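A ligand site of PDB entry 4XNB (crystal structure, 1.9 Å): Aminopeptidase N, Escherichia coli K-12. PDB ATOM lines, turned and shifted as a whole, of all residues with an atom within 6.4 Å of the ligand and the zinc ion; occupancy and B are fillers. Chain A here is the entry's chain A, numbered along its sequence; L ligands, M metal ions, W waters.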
ATOM      1  N   GLN A 115       7.293   8.263 -19.665  1.00  0.00           N
ATOM      2  CA  GLN A 115       8.731   8.342 -19.242  1.00  0.00           C
ATOM      3  C   GLN A 115       8.948   9.683 -18.623  1.00  0.00           C
ATOM      4  O   GLN A 115       8.745  10.734 -19.296  1.00  0.00           O
ATOM      5  CB  GLN A 115       9.634   8.131 -20.487  1.00  0.00           C
ATOM      6  CG  GLN A 115      11.114   8.344 -20.191  1.00  0.00           C
ATOM      7  CD  GLN A 115      11.590   7.458 -19.058  1.00  0.00           C
ATOM      8  OE1 GLN A 115      11.159   6.297 -18.939  1.00  0.00           O
ATOM      9  NE2 GLN A 115      12.459   7.973 -18.225  1.00  0.00           N
ATOM     10  N   GLU A 117      11.760  10.371 -16.197  1.00  0.00           N
ATOM     11  CA  GLU A 117      13.148  10.783 -15.918  1.00  0.00           C
ATOM     12  C   GLU A 117      13.725  11.432 -17.183  1.00  0.00           C
ATOM     13  O   GLU A 117      13.533  10.890 -18.246  1.00  0.00           O
ATOM     14  CB  GLU A 117      14.028   9.624 -15.480  1.00  0.00           C
ATOM     15  CG  GLU A 117      15.369  10.079 -14.949  1.00  0.00           C
ATOM     16  CD  GLU A 117      16.278   8.990 -14.422  1.00  0.00           C
ATOM     17  OE1 GLU A 117      15.791   7.848 -14.254  1.00  0.00           O
ATOM     18  OE2 GLU A 117      17.461   9.284 -14.119  1.00  0.00           O
ATOM     19  N   ALA A 118      14.433  12.580 -17.081  1.00  0.00           N
ATOM     20  CA  ALA A 118      14.711  13.315 -15.840  1.00  0.00           C
ATOM     21  C   ALA A 118      13.569  14.275 -15.465  1.00  0.00           C
ATOM     22  O   ALA A 118      13.125  14.326 -14.285  1.00  0.00           O
ATOM     23  CB  ALA A 118      16.033  14.125 -15.965  1.00  0.00           C
ATOM     24  N   TYR A 181      10.145  11.807 -10.912  1.00  0.00           N
ATOM     25  CA  TYR A 181      10.724  11.091 -12.031  1.00  0.00           C
ATOM     26  C   TYR A 181      10.469   9.599 -11.987  1.00  0.00           C
ATOM     27  O   TYR A 181      10.596   8.928 -13.033  1.00  0.00           O
ATOM     28  CB  TYR A 181      12.193  11.395 -12.229  1.00  0.00           C
ATOM     29  CG  TYR A 181      13.147  10.624 -11.319  1.00  0.00           C
ATOM     30  CD1 TYR A 181      13.682   9.424 -11.719  1.00  0.00           C
ATOM     31  CD2 TYR A 181      13.609  11.178 -10.095  1.00  0.00           C
ATOM     32  CE1 TYR A 181      14.551   8.719 -10.908  1.00  0.00           C
ATOM     33  CE2 TYR A 181      14.542  10.488  -9.302  1.00  0.00           C
ATOM     34  CZ  TYR A 181      14.970   9.228  -9.709  1.00  0.00           C
ATOM     35  OH  TYR A 181      15.839   8.516  -8.914  1.00  0.00           O
ATOM     36  N   PHE A 254      10.609   3.614 -27.185  1.00  0.00           N
ATOM     37  CA  PHE A 254      11.275   4.030 -25.989  1.00  0.00           C
ATOM     38  C   PHE A 254      12.644   4.614 -26.366  1.00  0.00           C
ATOM     39  O   PHE A 254      13.367   4.003 -27.155  1.00  0.00           O
ATOM     40  CB  PHE A 254      11.466   2.779 -25.089  1.00  0.00           C
ATOM     41  CG  PHE A 254      11.675   3.117 -23.653  1.00  0.00           C
ATOM     42  CD1 PHE A 254      10.606   3.613 -22.897  1.00  0.00           C
ATOM     43  CD2 PHE A 254      12.981   2.998 -23.052  1.00  0.00           C
ATOM     44  CE1 PHE A 254      10.771   3.939 -21.581  1.00  0.00           C
ATOM     45  CE2 PHE A 254      13.160   3.372 -21.724  1.00  0.00           C
ATOM     46  CZ  PHE A 254      12.049   3.820 -20.979  1.00  0.00           C
ATOM     47  N   ASN A 255      12.995   5.755 -25.776  1.00  0.00           N
ATOM     48  CA  ASN A 255      14.216   6.428 -26.094  1.00  0.00           C
ATOM     49  C   ASN A 255      15.507   5.833 -25.565  1.00  0.00           C
ATOM     50  O   ASN A 255      16.542   6.015 -26.191  1.00  0.00           O
ATOM     51  CB  ASN A 255      14.134   7.920 -25.713  1.00  0.00           C
ATOM     52  CG  ASN A 255      13.215   8.690 -26.660  1.00  0.00           C
ATOM     53  OD1 ASN A 255      12.945   8.264 -27.818  1.00  0.00           O
ATOM     54  ND2 ASN A 255      12.787   9.862 -26.188  1.00  0.00           N
ATOM     55  N   MET A 256      15.452   5.114 -24.437  1.00  0.00           N
ATOM     56  CA  MET A 256      16.666   4.462 -23.886  1.00  0.00           C
ATOM     57  C   MET A 256      16.462   2.995 -23.741  1.00  0.00           C
ATOM     58  O   MET A 256      15.762   2.389 -24.540  1.00  0.00           O
ATOM     59  CB  MET A 256      17.050   5.156 -22.561  1.00  0.00           C
ATOM     60  CG  MET A 256      17.233   6.647 -22.765  1.00  0.00           C
ATOM     61  SD  MET A 256      18.918   7.182 -22.399  1.00  0.00           S
ATOM     62  CE  MET A 256      19.263   6.280 -20.824  1.00  0.00           C
ATOM     63  N   GLY A 257      17.035   2.390 -22.744  1.00  0.00           N
ATOM     64  CA  GLY A 257      16.958   0.956 -22.563  1.00  0.00           C
ATOM     65  C   GLY A 257      15.784   0.592 -21.660  1.00  0.00           C
ATOM     66  O   GLY A 257      15.046  -0.320 -21.966  1.00  0.00           O
ATOM     67  N   ALA A 258      15.680   1.228 -20.513  1.00  0.00           N
ATOM     68  CA  ALA A 258      14.569   0.834 -19.611  1.00  0.00           C
ATOM     69  C   ALA A 258      14.507   1.885 -18.523  1.00  0.00           C
ATOM     70  O   ALA A 258      15.299   2.794 -18.540  1.00  0.00           O
ATOM     71  CB  ALA A 258      14.736  -0.577 -19.063  1.00  0.00           C
ATOM     72  N   MET A 259      13.588   1.755 -17.565  1.00  0.00           N
ATOM     73  CA  MET A 259      13.398   2.749 -16.534  1.00  0.00           C
ATOM     74  C   MET A 259      12.884   2.140 -15.223  1.00  0.00           C
ATOM     75  O   MET A 259      11.929   1.367 -15.253  1.00  0.00           O
ATOM     76  CB  MET A 259      12.460   3.795 -17.057  1.00  0.00           C
ATOM     77  CG  MET A 259      12.008   4.849 -16.060  1.00  0.00           C
ATOM     78  SD  MET A 259      13.483   5.866 -15.560  1.00  0.00           S
ATOM     79  CE  MET A 259      13.078   6.278 -13.876  1.00  0.00           C
ATOM     80  N   GLU A 260      13.501   2.536 -14.112  1.00  0.00           N
ATOM     81  CA  GLU A 260      13.327   1.892 -12.827  1.00  0.00           C
ATOM     82  C   GLU A 260      12.117   2.417 -12.019  1.00  0.00           C
ATOM     83  O   GLU A 260      12.211   2.458 -10.801  1.00  0.00           O
ATOM     84  CB  GLU A 260      14.557   2.042 -11.977  1.00  0.00           C
ATOM     85  CG  GLU A 260      14.942   3.465 -11.529  1.00  0.00           C
ATOM     86  CD  GLU A 260      15.868   4.259 -12.506  1.00  0.00           C
ATOM     87  OE1 GLU A 260      15.943   3.939 -13.721  1.00  0.00           O
ATOM     88  OE2 GLU A 260      16.473   5.268 -12.009  1.00  0.00           O
ATOM     89  N   HIS A 293      19.966  -4.275 -13.806  1.00  0.00           N
ATOM     90  CA  HIS A 293      20.159  -2.850 -13.611  1.00  0.00           C
ATOM     91  C   HIS A 293      18.925  -2.153 -13.045  1.00  0.00           C
ATOM     92  O   HIS A 293      19.018  -1.458 -12.016  1.00  0.00           O
ATOM     93  CB  HIS A 293      20.587  -2.209 -14.971  1.00  0.00           C
ATOM     94  CG  HIS A 293      20.969  -0.776 -14.856  1.00  0.00           C
ATOM     95  ND1 HIS A 293      22.251  -0.354 -14.653  1.00  0.00           N
ATOM     96  CD2 HIS A 293      20.206   0.340 -14.868  1.00  0.00           C
ATOM     97  CE1 HIS A 293      22.280   0.958 -14.507  1.00  0.00           C
ATOM     98  NE2 HIS A 293      21.035   1.408 -14.649  1.00  0.00           N
ATOM     99  N   GLU A 294      17.775  -2.267 -13.705  1.00  0.00           N
ATOM    100  CA  GLU A 294      16.569  -1.582 -13.215  1.00  0.00           C
ATOM    101  C   GLU A 294      16.198  -2.090 -11.808  1.00  0.00           C
ATOM    102  O   GLU A 294      15.780  -1.335 -10.979  1.00  0.00           O
ATOM    103  CB  GLU A 294      15.395  -1.646 -14.204  1.00  0.00           C
ATOM    104  CG  GLU A 294      15.801  -1.333 -15.652  1.00  0.00           C
ATOM    105  CD  GLU A 294      16.578  -0.014 -15.830  1.00  0.00           C
ATOM    106  OE1 GLU A 294      16.279   0.928 -15.095  1.00  0.00           O
ATOM    107  OE2 GLU A 294      17.391   0.078 -16.760  1.00  0.00           O
ATOM    108  N   HIS A 297      18.354  -0.538  -9.085  1.00  0.00           N
ATOM    109  CA  HIS A 297      17.975   0.816  -8.765  1.00  0.00           C
ATOM    110  C   HIS A 297      16.930   0.895  -7.653  1.00  0.00           C
ATOM    111  O   HIS A 297      16.750   1.928  -7.078  1.00  0.00           O
ATOM    112  CB  HIS A 297      17.336   1.490 -10.000  1.00  0.00           C
ATOM    113  CG  HIS A 297      18.291   2.231 -10.888  1.00  0.00           C
ATOM    114  ND1 HIS A 297      19.186   3.151 -10.407  1.00  0.00           N
ATOM    115  CD2 HIS A 297      18.437   2.233 -12.243  1.00  0.00           C
ATOM    116  CE1 HIS A 297      19.822   3.707 -11.419  1.00  0.00           C
ATOM    117  NE2 HIS A 297      19.382   3.164 -12.517  1.00  0.00           N
ATOM    118  N   LEU A 312      23.441  12.621 -10.638  1.00  0.00           N
ATOM    119  CA  LEU A 312      22.990  11.477 -11.345  1.00  0.00           C
ATOM    120  C   LEU A 312      23.890  10.237 -11.167  1.00  0.00           C
ATOM    121  O   LEU A 312      23.375   9.121 -10.978  1.00  0.00           O
ATOM    122  CB  LEU A 312      22.816  11.797 -12.859  1.00  0.00           C
ATOM    123  CG  LEU A 312      22.343  10.643 -13.735  1.00  0.00           C
ATOM    124  CD1 LEU A 312      20.946  10.140 -13.309  1.00  0.00           C
ATOM    125  CD2 LEU A 312      22.297  11.040 -15.145  1.00  0.00           C
ATOM    126  N   LYS A 315      23.380   7.408  -8.399  1.00  0.00           N
ATOM    127  CA  LYS A 315      22.614   6.243  -8.722  1.00  0.00           C
ATOM    128  C   LYS A 315      23.121   5.506  -9.962  1.00  0.00           C
ATOM    129  O   LYS A 315      23.100   4.271  -9.966  1.00  0.00           O
ATOM    130  CB  LYS A 315      21.093   6.521  -8.795  1.00  0.00           C
ATOM    131  CG  LYS A 315      20.589   7.346  -9.973  1.00  0.00           C
ATOM    132  CD  LYS A 315      19.070   7.558  -9.902  1.00  0.00           C
ATOM    133  CE  LYS A 315      18.410   8.273 -11.090  1.00  0.00           C
ATOM    134  NZ  LYS A 315      18.288   7.515 -12.324  1.00  0.00           N
ATOM    135  N   GLU A 316      23.587   6.211 -10.994  1.00  0.00           N
ATOM    136  CA  GLU A 316      23.945   5.521 -12.214  1.00  0.00           C
ATOM    137  C   GLU A 316      25.311   4.802 -12.146  1.00  0.00           C
ATOM    138  O   GLU A 316      25.420   3.663 -12.586  1.00  0.00           O
ATOM    139  CB  GLU A 316      23.795   6.382 -13.458  1.00  0.00           C
ATOM    140  CG  GLU A 316      22.378   6.891 -13.716  1.00  0.00           C
ATOM    141  CD  GLU A 316      21.373   5.792 -13.847  1.00  0.00           C
ATOM    142  OE1 GLU A 316      21.810   4.645 -14.000  1.00  0.00           O
ATOM    143  OE2 GLU A 316      20.165   6.088 -13.700  1.00  0.00           O
ATOM    144  N   THR A 319      24.714   1.852  -9.727  1.00  0.00           N
ATOM    145  CA  THR A 319      23.847   0.799 -10.298  1.00  0.00           C
ATOM    146  C   THR A 319      24.510   0.068 -11.480  1.00  0.00           C
ATOM    147  O   THR A 319      24.338  -1.114 -11.652  1.00  0.00           O
ATOM    148  CB  THR A 319      22.437   1.333 -10.616  1.00  0.00           C
ATOM    149  OG1 THR A 319      21.916   1.957  -9.418  1.00  0.00           O
ATOM    150  CG2 THR A 319      21.542   0.251 -11.151  1.00  0.00           C
ATOM    151  N   VAL A 320      25.260   0.804 -12.303  1.00  0.00           N
ATOM    152  CA  VAL A 320      26.094   0.130 -13.297  1.00  0.00           C
ATOM    153  C   VAL A 320      27.159  -0.772 -12.652  1.00  0.00           C
ATOM    154  O   VAL A 320      27.361  -1.902 -13.084  1.00  0.00           O
ATOM    155  CB  VAL A 320      26.822   1.125 -14.253  1.00  0.00           C
ATOM    156  CG1 VAL A 320      27.855   0.361 -15.096  1.00  0.00           C
ATOM    157  CG2 VAL A 320      25.847   1.887 -15.129  1.00  0.00           C
ATOM    158  N   ASN A 369      18.871  15.788 -20.253  1.00  0.00           N
ATOM    159  CA  ASN A 369      18.865  14.523 -21.014  1.00  0.00           C
ATOM    160  C   ASN A 369      20.111  14.289 -21.831  1.00  0.00           C
ATOM    161  O   ASN A 369      20.356  13.132 -22.196  1.00  0.00           O
ATOM    162  CB  ASN A 369      17.678  14.397 -21.917  1.00  0.00           C
ATOM    163  CG  ASN A 369      16.333  14.236 -21.124  1.00  0.00           C
ATOM    164  OD1 ASN A 369      16.242  13.577 -20.032  1.00  0.00           O
ATOM    165  ND2 ASN A 369      15.282  14.845 -21.709  1.00  0.00           N
ATOM    166  N   TYR A 372      22.998  11.668 -19.729  1.00  0.00           N
ATOM    167  CA  TYR A 372      22.886  10.212 -19.502  1.00  0.00           C
ATOM    168  C   TYR A 372      23.997   9.564 -20.310  1.00  0.00           C
ATOM    169  O   TYR A 372      23.763   8.956 -21.316  1.00  0.00           O
ATOM    170  CB  TYR A 372      21.462   9.740 -19.876  1.00  0.00           C
ATOM    171  CG  TYR A 372      20.537  10.191 -18.769  1.00  0.00           C
ATOM    172  CD1 TYR A 372      20.042  11.508 -18.719  1.00  0.00           C
ATOM    173  CD2 TYR A 372      20.163   9.336 -17.752  1.00  0.00           C
ATOM    174  CE1 TYR A 372      19.315  11.959 -17.613  1.00  0.00           C
ATOM    175  CE2 TYR A 372      19.422   9.773 -16.635  1.00  0.00           C
ATOM    176  CZ  TYR A 372      18.962  11.099 -16.620  1.00  0.00           C
ATOM    177  OH  TYR A 372      18.235  11.501 -15.525  1.00  0.00           O
ATOM    178  N   TYR A 377      27.683   7.058 -16.416  1.00  0.00           N
ATOM    179  CA  TYR A 377      27.380   5.608 -16.209  1.00  0.00           C
ATOM    180  C   TYR A 377      28.668   4.760 -16.077  1.00  0.00           C
ATOM    181  O   TYR A 377      28.980   4.220 -15.010  1.00  0.00           O
ATOM    182  CB  TYR A 377      26.537   5.102 -17.375  1.00  0.00           C
ATOM    183  CG  TYR A 377      25.081   5.423 -17.285  1.00  0.00           C
ATOM    184  CD1 TYR A 377      24.585   6.719 -17.401  1.00  0.00           C
ATOM    185  CD2 TYR A 377      24.127   4.360 -17.182  1.00  0.00           C
ATOM    186  CE1 TYR A 377      23.200   6.968 -17.315  1.00  0.00           C
ATOM    187  CE2 TYR A 377      22.763   4.617 -17.130  1.00  0.00           C
ATOM    188  CZ  TYR A 377      22.303   5.911 -17.195  1.00  0.00           C
ATOM    189  OH  TYR A 377      20.903   6.134 -17.087  1.00  0.00           O
ATOM    190  N   GLN A 817      15.693  13.962 -28.110  1.00  0.00           N
ATOM    191  CA  GLN A 817      16.575  13.086 -27.399  1.00  0.00           C
ATOM    192  C   GLN A 817      17.332  12.147 -28.320  1.00  0.00           C
ATOM    193  O   GLN A 817      18.507  11.944 -28.174  1.00  0.00           O
ATOM    194  CB  GLN A 817      15.848  12.249 -26.332  1.00  0.00           C
ATOM    195  CG  GLN A 817      15.553  13.120 -25.177  1.00  0.00           C
ATOM    196  CD  GLN A 817      14.698  12.387 -24.069  1.00  0.00           C
ATOM    197  OE1 GLN A 817      15.006  11.281 -23.636  1.00  0.00           O
ATOM    198  NE2 GLN A 817      13.669  13.009 -23.661  1.00  0.00           N
HETATM  199  N1  LIG L   1      17.284   5.808 -15.100  1.00  0.00           N
HETATM  200  C1  LIG L   1      16.919   5.548 -16.516  1.00  0.00           C
HETATM  201  C2  LIG L   1      17.267   6.853 -17.305  1.00  0.00           C
HETATM  202  C3  LIG L   1      16.395   7.210 -18.463  1.00  0.00           C
HETATM  203  C4  LIG L   1      16.463   8.538 -18.881  1.00  0.00           C
HETATM  204  C5  LIG L   1      15.698   8.874 -19.994  1.00  0.00           C
HETATM  205  C6  LIG L   1      14.880   7.989 -20.663  1.00  0.00           C
HETATM  206  C7  LIG L   1      14.812   6.665 -20.216  1.00  0.00           C
HETATM  207  C8  LIG L   1      15.584   6.295 -19.133  1.00  0.00           C
HETATM  208  C9  LIG L   1      17.621   4.387 -17.242  1.00  0.00           C
HETATM  209  C10 LIG L   1      18.534   3.729 -16.246  1.00  0.00           C
HETATM  210  O1  LIG L   1      19.653   4.145 -16.021  1.00  0.00           O
HETATM  211  O2  LIG L   1      18.065   2.796 -15.502  1.00  0.00           O
HETATM  212 ZN    ZN M   1      20.365   3.331 -14.340  1.00  0.00          ZN
HETATM  213  O   HOH W   1      13.066   6.622 -23.009  1.00  0.00           O
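The side-chain hydroxyl (OH) of Tyr 377 sits close to an oxygen (O1) of the ligand, 2.6 Å away. A nitrogen (N1) of the ligand is in salt-bridge range of the side-chain carboxylate (OE1) of Glu 117 (2.7 Å). The side-chain amino group (NZ) of Lys 315 sits close to a nitrogen (N1) of the ligand (3.4 Å). The side-chain carboxylate (OE1) of Glu 260 is in salt-bridge range of a nitrogen (N1) of the ligand. An oxygen (O2) of the ligand lies close to the side-chain carboxylate (OE1) of Glu 294.
NE2 of Gln 115 sits at hydrogen-bond distance from O of Glu 117 (3.1 Å). OE2 of Glu 117 lies within hydrogen-bond range of OH of Tyr 372, 2.7 Å away. A ring nitrogen (ND1) of His 297 is in hydrogen-bond range of the side-chain hydroxyl (OG1) of Thr 319 (3.1 Å). N of Glu 260 is in hydrogen-bond range of OE1 of Glu 294 (3.4 Å). The side-chain carboxylate of Glu 316 lies within salt-bridge range of the side-chain amino group of Lys 315 (2.7 Å). The side-chain amide nitrogen (NE2) of Gln 115 sits at hydrogen-bond distance from the side-chain sulfur (SD) of Met 259 (3.5 Å). The backbone carbonyl oxygen (O) of Lys 315 sits at hydrogen-bond distance from the side-chain hydroxyl (OG1) of Thr 319. OE2 of Glu 316 sits close to OH of Tyr 377 (3.5 Å).
Gln 115 touches the ligand (NE2 to C7, 3.3 Å). Phe 254 touches the ligand. CG of Met 256 touches C6 of the ligand (3.4 Å). Ala 258 touches the ligand. SD of Met 259 touches C1 of the ligand, 3.6 Å away. CE2 of Tyr 372 touches C2 of the ligand, 3.7 Å away. Hydrophobic or aromatic side chains within 4 Å of the ligand: Phe 254, Met 256, Met 259, His 293, His 297, Tyr 372 and Tyr 377. Of the 23 residues printed, 14 come within 4 Å of the ligand. The nearest printed residue that does not touch the ligand is Gln 817 (4.4 Å).
Merely in contact with the zinc ion: Tyr 377 (3.9 Å). Four residues have an atom within 4 Å of the zinc ion: His 293, His 297, Glu 316 and Tyr 377.
The zinc ion is bound by OE1 of Glu 316, O1 of the ligand, NE2 of His 293 and NE2 of His 297. Slightly farther from the zinc ion lies O2 of the ligand (2.6 Å). Slightly farther from the zinc ion lies OE2 of Glu 316 (2.8 Å).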
